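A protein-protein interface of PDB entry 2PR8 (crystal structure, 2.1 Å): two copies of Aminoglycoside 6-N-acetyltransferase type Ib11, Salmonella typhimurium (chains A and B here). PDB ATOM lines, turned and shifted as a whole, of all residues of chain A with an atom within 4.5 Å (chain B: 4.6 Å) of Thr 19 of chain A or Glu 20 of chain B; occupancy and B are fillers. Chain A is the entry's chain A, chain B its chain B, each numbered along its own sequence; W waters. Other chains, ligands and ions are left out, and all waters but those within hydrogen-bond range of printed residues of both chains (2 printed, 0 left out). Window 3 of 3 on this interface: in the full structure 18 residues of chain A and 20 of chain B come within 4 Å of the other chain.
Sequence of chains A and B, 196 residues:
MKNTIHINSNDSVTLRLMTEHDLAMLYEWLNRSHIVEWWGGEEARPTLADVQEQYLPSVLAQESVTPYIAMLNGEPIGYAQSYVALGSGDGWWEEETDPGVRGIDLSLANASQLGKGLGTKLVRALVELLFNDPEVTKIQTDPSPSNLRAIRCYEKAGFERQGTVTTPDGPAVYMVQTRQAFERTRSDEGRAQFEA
Water W1 lies within hydrogen-bond range of OE1 of Glu 20 of chain B (2.6 Å), OG1 of Thr 19 of chain A (2.8 Å), N of His 21 of chain A (2.9 Å) and N of Glu 20 of chain A (3.5 Å).
Water W2 lies within hydrogen-bond range of OG1 of Thr 19 of chain B, OE1 of Glu 20 of chain A and N of His 21 of chain B.
OG of Ser 58 of chain B lies within hydrogen-bond range of O of Met 18 of chain A, at 2.5 Å.
The backbone NH (N) of Glu 20 of chain A is in hydrogen-bond range of the side-chain carboxylate (OE2) of Glu 20 of chain B, 2.8 Å away.
Thr 19 of chain A touches Glu 20 of chain B, and with the chains exchanged Glu 20 of chain A touches Thr 19 of chain B.
Glu 20 of chain B touches its own counterpart, Glu 20 of chain A.
5 positions are printed for both chains.
Of the 5 pairs that touch across the chains among the printed residues, 3 have their exchanged pair printed and touching as well.
Leu 17 of chain A touches none of the printed residues of chain B.
Of the printed residues of chain B, Met 18 of chain A touches Ser 58.
Printed residues of chain B within 4 Å of Thr 19 of chain A: Glu 20 and Ser 58.
Printed residues of chain B within 4 Å of Glu 20 of chain A: Thr 19 and Glu 20.
Of the printed residues of chain A, Thr 19 of chain B touches Glu 20.
Printed residues of chain A within 4 Å of Glu 20 of chain B: Thr 19 (3.3 Å) and Glu 20 (2.8 Å).
Of the printed residues of chain A, Ser 58 of chain B touches Met 18 and Thr 19.
The nearest printed residue of chain B that does not touch Thr 19 of chain A is Leu 56 of chain B (4.1 Å).
The nearest printed residue of chain A that does not touch Thr 19 of chain B is Leu 23 of chain A (8.0 Å).
Of the 8 printed residues of chain B, 3 touch a printed residue of chain A.
Printed residues of chain B that touch a printed residue of chain A: Thr 19, Glu 20 and Ser 58.
Along chain B the printed residues that touch a printed residue of chain A span positions 19 to 58.
Of the 8 printed residues of chain A, 3 touch a printed residue of chain B.
Among the printed residues, no Asp or Glu carboxylate lies within 4 Å of a Lys or Arg side-chain nitrogen of the other chain.
OD2 of Asp 22 of chain A lies within hydrogen-bond range of N of Thr 19 of chain A, 2.7 Å away.
The side-chain hydroxyl (OG1) of Thr 19 of chain B lies close to the backbone NH (N) of His 21 of chain B (3.5 Å).
The backbone NH (N) of Thr 19 of chain B sits at hydrogen-bond distance from the side-chain carboxylate (OD2) of Asp 22 of chain B (2.8 Å).
Among the printed residues, merely in contact across the chains: Thr 19 of chain A with Glu 20 of chain B, Glu 20 of chain A with Thr 19 of chain B and Thr 19 of chain A with Ser 58 of chain B.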
ATOM      1  N   ARG A  16      -8.125 -22.080 -13.116  1.00  0.00           N
ATOM      2  CA  ARG A  16      -7.856 -20.824 -12.464  1.00  0.00           C
ATOM      3  C   ARG A  16      -9.014 -20.513 -11.539  1.00  0.00           C
ATOM      4  O   ARG A  16     -10.107 -21.100 -11.658  1.00  0.00           O
ATOM      5  CB  ARG A  16      -7.686 -19.701 -13.513  1.00  0.00           C
ATOM      6  CG  ARG A  16      -8.978 -19.328 -14.292  1.00  0.00           C
ATOM      7  CD  ARG A  16      -8.698 -18.208 -15.279  1.00  0.00           C
ATOM      8  NE  ARG A  16      -9.821 -17.868 -16.158  1.00  0.00           N
ATOM      9  CZ  ARG A  16     -10.972 -17.302 -15.793  1.00  0.00           C
ATOM     10  NH1 ARG A  16     -11.873 -17.017 -16.731  1.00  0.00           N
ATOM     11  NH2 ARG A  16     -11.238 -17.002 -14.520  1.00  0.00           N
ATOM     12  N   LEU A  17      -8.783 -19.569 -10.633  1.00  0.00           N
ATOM     13  CA  LEU A  17      -9.823 -19.025  -9.827  1.00  0.00           C
ATOM     14  C   LEU A  17     -10.834 -18.352 -10.724  1.00  0.00           C
ATOM     15  O   LEU A  17     -10.462 -17.625 -11.660  1.00  0.00           O
ATOM     16  CB  LEU A  17      -9.254 -18.010  -8.817  1.00  0.00           C
ATOM     17  CG  LEU A  17      -8.458 -18.620  -7.652  1.00  0.00           C
ATOM     18  CD1 LEU A  17      -7.863 -17.499  -6.701  1.00  0.00           C
ATOM     19  CD2 LEU A  17      -9.350 -19.590  -6.864  1.00  0.00           C
ATOM     20  N   MET A  18     -12.115 -18.597 -10.424  1.00  0.00           N
ATOM     21  CA  MET A  18     -13.188 -17.893 -11.067  1.00  0.00           C
ATOM     22  C   MET A  18     -13.261 -16.508 -10.436  1.00  0.00           C
ATOM     23  O   MET A  18     -13.107 -16.363  -9.231  1.00  0.00           O
ATOM     24  CB  MET A  18     -14.520 -18.621 -10.888  1.00  0.00           C
ATOM     25  CG  MET A  18     -15.639 -17.968 -11.659  1.00  0.00           C
ATOM     26  SD  MET A  18     -17.256 -18.052 -10.909  1.00  0.00           S
ATOM     27  CE  MET A  18     -18.291 -17.879 -12.330  1.00  0.00           C
ATOM     28  N   THR A  19     -13.531 -15.502 -11.248  1.00  0.00           N
ATOM     29  CA  THR A  19     -13.659 -14.133 -10.735  1.00  0.00           C
ATOM     30  C   THR A  19     -14.994 -13.598 -11.168  1.00  0.00           C
ATOM     31  O   THR A  19     -15.696 -14.267 -11.935  1.00  0.00           O
ATOM     32  CB  THR A  19     -12.498 -13.211 -11.201  1.00  0.00           C
ATOM     33  OG1 THR A  19     -12.542 -13.057 -12.614  1.00  0.00           O
ATOM     34  CG2 THR A  19     -11.153 -13.784 -10.789  1.00  0.00           C
ATOM     35  N   GLU A  20     -15.359 -12.406 -10.697  1.00  0.00           N
ATOM     36  CA  GLU A  20     -16.690 -11.891 -10.987  1.00  0.00           C
ATOM     37  C   GLU A  20     -16.949 -11.667 -12.472  1.00  0.00           C
ATOM     38  O   GLU A  20     -18.045 -11.895 -12.967  1.00  0.00           O
ATOM     39  CB  GLU A  20     -16.948 -10.651 -10.207  1.00  0.00           C
ATOM     40  CG  GLU A  20     -17.127 -10.985  -8.768  1.00  0.00           C
ATOM     41  CD  GLU A  20     -17.428  -9.757  -7.955  1.00  0.00           C
ATOM     42  OE1 GLU A  20     -17.953  -8.799  -8.529  1.00  0.00           O
ATOM     43  OE2 GLU A  20     -17.170  -9.767  -6.746  1.00  0.00           O
ATOM     44  N   HIS A  21     -15.910 -11.306 -13.210  1.00  0.00           N
ATOM     45  CA  HIS A  21     -16.098 -11.190 -14.646  1.00  0.00           C
ATOM     46  C   HIS A  21     -16.619 -12.495 -15.280  1.00  0.00           C
ATOM     47  O   HIS A  21     -17.301 -12.454 -16.289  1.00  0.00           O
ATOM     48  CB  HIS A  21     -14.826 -10.699 -15.353  1.00  0.00           C
ATOM     49  CG  HIS A  21     -14.940 -10.738 -16.847  1.00  0.00           C
ATOM     50  ND1 HIS A  21     -14.249 -11.644 -17.624  1.00  0.00           N
ATOM     51  CD2 HIS A  21     -15.715 -10.026 -17.696  1.00  0.00           C
ATOM     52  CE1 HIS A  21     -14.567 -11.460 -18.894  1.00  0.00           C
ATOM     53  NE2 HIS A  21     -15.452 -10.480 -18.964  1.00  0.00           N
ATOM     54  N   ASP A  22     -16.345 -13.634 -14.654  1.00  0.00           N
ATOM     55  CA  ASP A  22     -16.797 -14.920 -15.168  1.00  0.00           C
ATOM     56  C   ASP A  22     -18.274 -15.186 -14.949  1.00  0.00           C
ATOM     57  O   ASP A  22     -18.825 -16.127 -15.521  1.00  0.00           O
ATOM     58  CB  ASP A  22     -15.985 -16.053 -14.547  1.00  0.00           C
ATOM     59  CG  ASP A  22     -14.513 -15.883 -14.786  1.00  0.00           C
ATOM     60  OD1 ASP A  22     -14.138 -15.475 -15.927  1.00  0.00           O
ATOM     61  OD2 ASP A  22     -13.736 -16.126 -13.830  1.00  0.00           O
ATOM     62  N   LEU A  23     -18.914 -14.375 -14.123  1.00  0.00           N
ATOM     63  CA  LEU A  23     -20.295 -14.650 -13.766  1.00  0.00           C
ATOM     64  C   LEU A  23     -21.247 -14.535 -14.971  1.00  0.00           C
ATOM     65  O   LEU A  23     -22.172 -15.359 -15.099  1.00  0.00           O
ATOM     66  CB  LEU A  23     -20.756 -13.780 -12.606  1.00  0.00           C
ATOM     67  CG  LEU A  23     -20.195 -13.998 -11.192  1.00  0.00           C
ATOM     68  CD1 LEU A  23     -20.654 -12.834 -10.305  1.00  0.00           C
ATOM     69  CD2 LEU A  23     -20.586 -15.357 -10.566  1.00  0.00           C
ATOM     70  N   THR B  19     -17.292  -6.844  -2.956  1.00  0.00           N
ATOM     71  CA  THR B  19     -17.231  -7.416  -4.317  1.00  0.00           C
ATOM     72  C   THR B  19     -16.014  -6.835  -5.000  1.00  0.00           C
ATOM     73  O   THR B  19     -15.348  -5.970  -4.454  1.00  0.00           O
ATOM     74  CB  THR B  19     -18.490  -7.089  -5.189  1.00  0.00           C
ATOM     75  OG1 THR B  19     -18.463  -5.696  -5.533  1.00  0.00           O
ATOM     76  CG2 THR B  19     -19.804  -7.455  -4.490  1.00  0.00           C
ATOM     77  N   GLU B  20     -15.714  -7.297  -6.197  1.00  0.00           N
ATOM     78  CA  GLU B  20     -14.510  -6.816  -6.871  1.00  0.00           C
ATOM     79  C   GLU B  20     -14.511  -5.318  -7.151  1.00  0.00           C
ATOM     80  O   GLU B  20     -13.458  -4.664  -7.122  1.00  0.00           O
ATOM     81  CB  GLU B  20     -14.260  -7.597  -8.159  1.00  0.00           C
ATOM     82  CG  GLU B  20     -13.691  -8.989  -7.852  1.00  0.00           C
ATOM     83  CD  GLU B  20     -13.598  -9.846  -9.084  1.00  0.00           C
ATOM     84  OE1 GLU B  20     -13.502  -9.261 -10.190  1.00  0.00           O
ATOM     85  OE2 GLU B  20     -13.606 -11.097  -8.941  1.00  0.00           O
ATOM     86  N   HIS B  21     -15.697  -4.788  -7.416  1.00  0.00           N
ATOM     87  CA  HIS B  21     -15.889  -3.374  -7.648  1.00  0.00           C
ATOM     88  C   HIS B  21     -15.309  -2.546  -6.501  1.00  0.00           C
ATOM     89  O   HIS B  21     -14.761  -1.450  -6.722  1.00  0.00           O
ATOM     90  CB  HIS B  21     -17.382  -3.082  -7.839  1.00  0.00           C
ATOM     91  CG  HIS B  21     -17.669  -1.913  -8.742  1.00  0.00           C
ATOM     92  ND1 HIS B  21     -17.020  -1.721  -9.945  1.00  0.00           N
ATOM     93  CD2 HIS B  21     -18.561  -0.900  -8.629  1.00  0.00           C
ATOM     94  CE1 HIS B  21     -17.493  -0.634 -10.531  1.00  0.00           C
ATOM     95  NE2 HIS B  21     -18.428  -0.115  -9.751  1.00  0.00           N
ATOM     96  N   ASP B  22     -15.368  -3.082  -5.284  1.00  0.00           N
ATOM     97  CA  ASP B  22     -14.899  -2.358  -4.088  1.00  0.00           C
ATOM     98  C   ASP B  22     -13.392  -2.311  -3.917  1.00  0.00           C
ATOM     99  O   ASP B  22     -12.896  -1.611  -3.036  1.00  0.00           O
ATOM    100  CB  ASP B  22     -15.470  -3.000  -2.827  1.00  0.00           C
ATOM    101  CG  ASP B  22     -16.981  -3.022  -2.808  1.00  0.00           C
ATOM    102  OD1 ASP B  22     -17.621  -1.979  -3.101  1.00  0.00           O
ATOM    103  OD2 ASP B  22     -17.554  -4.069  -2.435  1.00  0.00           O
ATOM    104  N   LEU B  23     -12.654  -3.085  -4.710  1.00  0.00           N
ATOM    105  CA  LEU B  23     -11.222  -3.201  -4.507  1.00  0.00           C
ATOM    106  C   LEU B  23     -10.454  -1.909  -4.689  1.00  0.00           C
ATOM    107  O   LEU B  23      -9.477  -1.691  -3.989  1.00  0.00           O
ATOM    108  CB  LEU B  23     -10.600  -4.278  -5.423  1.00  0.00           C
ATOM    109  CG  LEU B  23     -10.919  -5.717  -4.961  1.00  0.00           C
ATOM    110  CD1 LEU B  23     -10.655  -6.704  -6.034  1.00  0.00           C
ATOM    111  CD2 LEU B  23     -10.126  -6.055  -3.694  1.00  0.00           C
ATOM    112  N   LEU B  56      -8.709  -9.956  -3.403  1.00  0.00           N
ATOM    113  CA  LEU B  56      -9.639 -10.546  -4.355  1.00  0.00           C
ATOM    114  C   LEU B  56     -10.534 -11.536  -3.640  1.00  0.00           C
ATOM    115  O   LEU B  56     -10.041 -12.493  -3.020  1.00  0.00           O
ATOM    116  CB  LEU B  56      -8.889 -11.262  -5.482  1.00  0.00           C
ATOM    117  CG  LEU B  56      -9.792 -11.738  -6.606  1.00  0.00           C
ATOM    118  CD1 LEU B  56     -10.244 -10.524  -7.469  1.00  0.00           C
ATOM    119  CD2 LEU B  56      -9.059 -12.746  -7.442  1.00  0.00           C
ATOM    120  N   PRO B  57     -11.857 -11.317  -3.684  1.00  0.00           N
ATOM    121  CA  PRO B  57     -12.695 -12.264  -2.952  1.00  0.00           C
ATOM    122  C   PRO B  57     -12.460 -13.763  -3.234  1.00  0.00           C
ATOM    123  O   PRO B  57     -12.536 -14.564  -2.306  1.00  0.00           O
ATOM    124  CB  PRO B  57     -14.104 -11.819  -3.328  1.00  0.00           C
ATOM    125  CG  PRO B  57     -13.920 -10.308  -3.493  1.00  0.00           C
ATOM    126  CD  PRO B  57     -12.653 -10.228  -4.271  1.00  0.00           C
ATOM    127  N   SER B  58     -12.181 -14.155  -4.484  1.00  0.00           N
ATOM    128  CA  SER B  58     -11.921 -15.584  -4.776  1.00  0.00           C
ATOM    129  C   SER B  58     -10.670 -16.083  -4.051  1.00  0.00           C
ATOM    130  O   SER B  58     -10.615 -17.262  -3.650  1.00  0.00           O
ATOM    131  CB  SER B  58     -11.770 -15.819  -6.290  1.00  0.00           C
ATOM    132  OG  SER B  58     -12.881 -15.275  -6.999  1.00  0.00           O
HETATM  133  O   HOH W   1     -13.223 -10.332 -12.507  1.00  0.00           O
HETATM  134  O   HOH W   2     -18.404  -5.939  -8.100  1.00  0.00           O
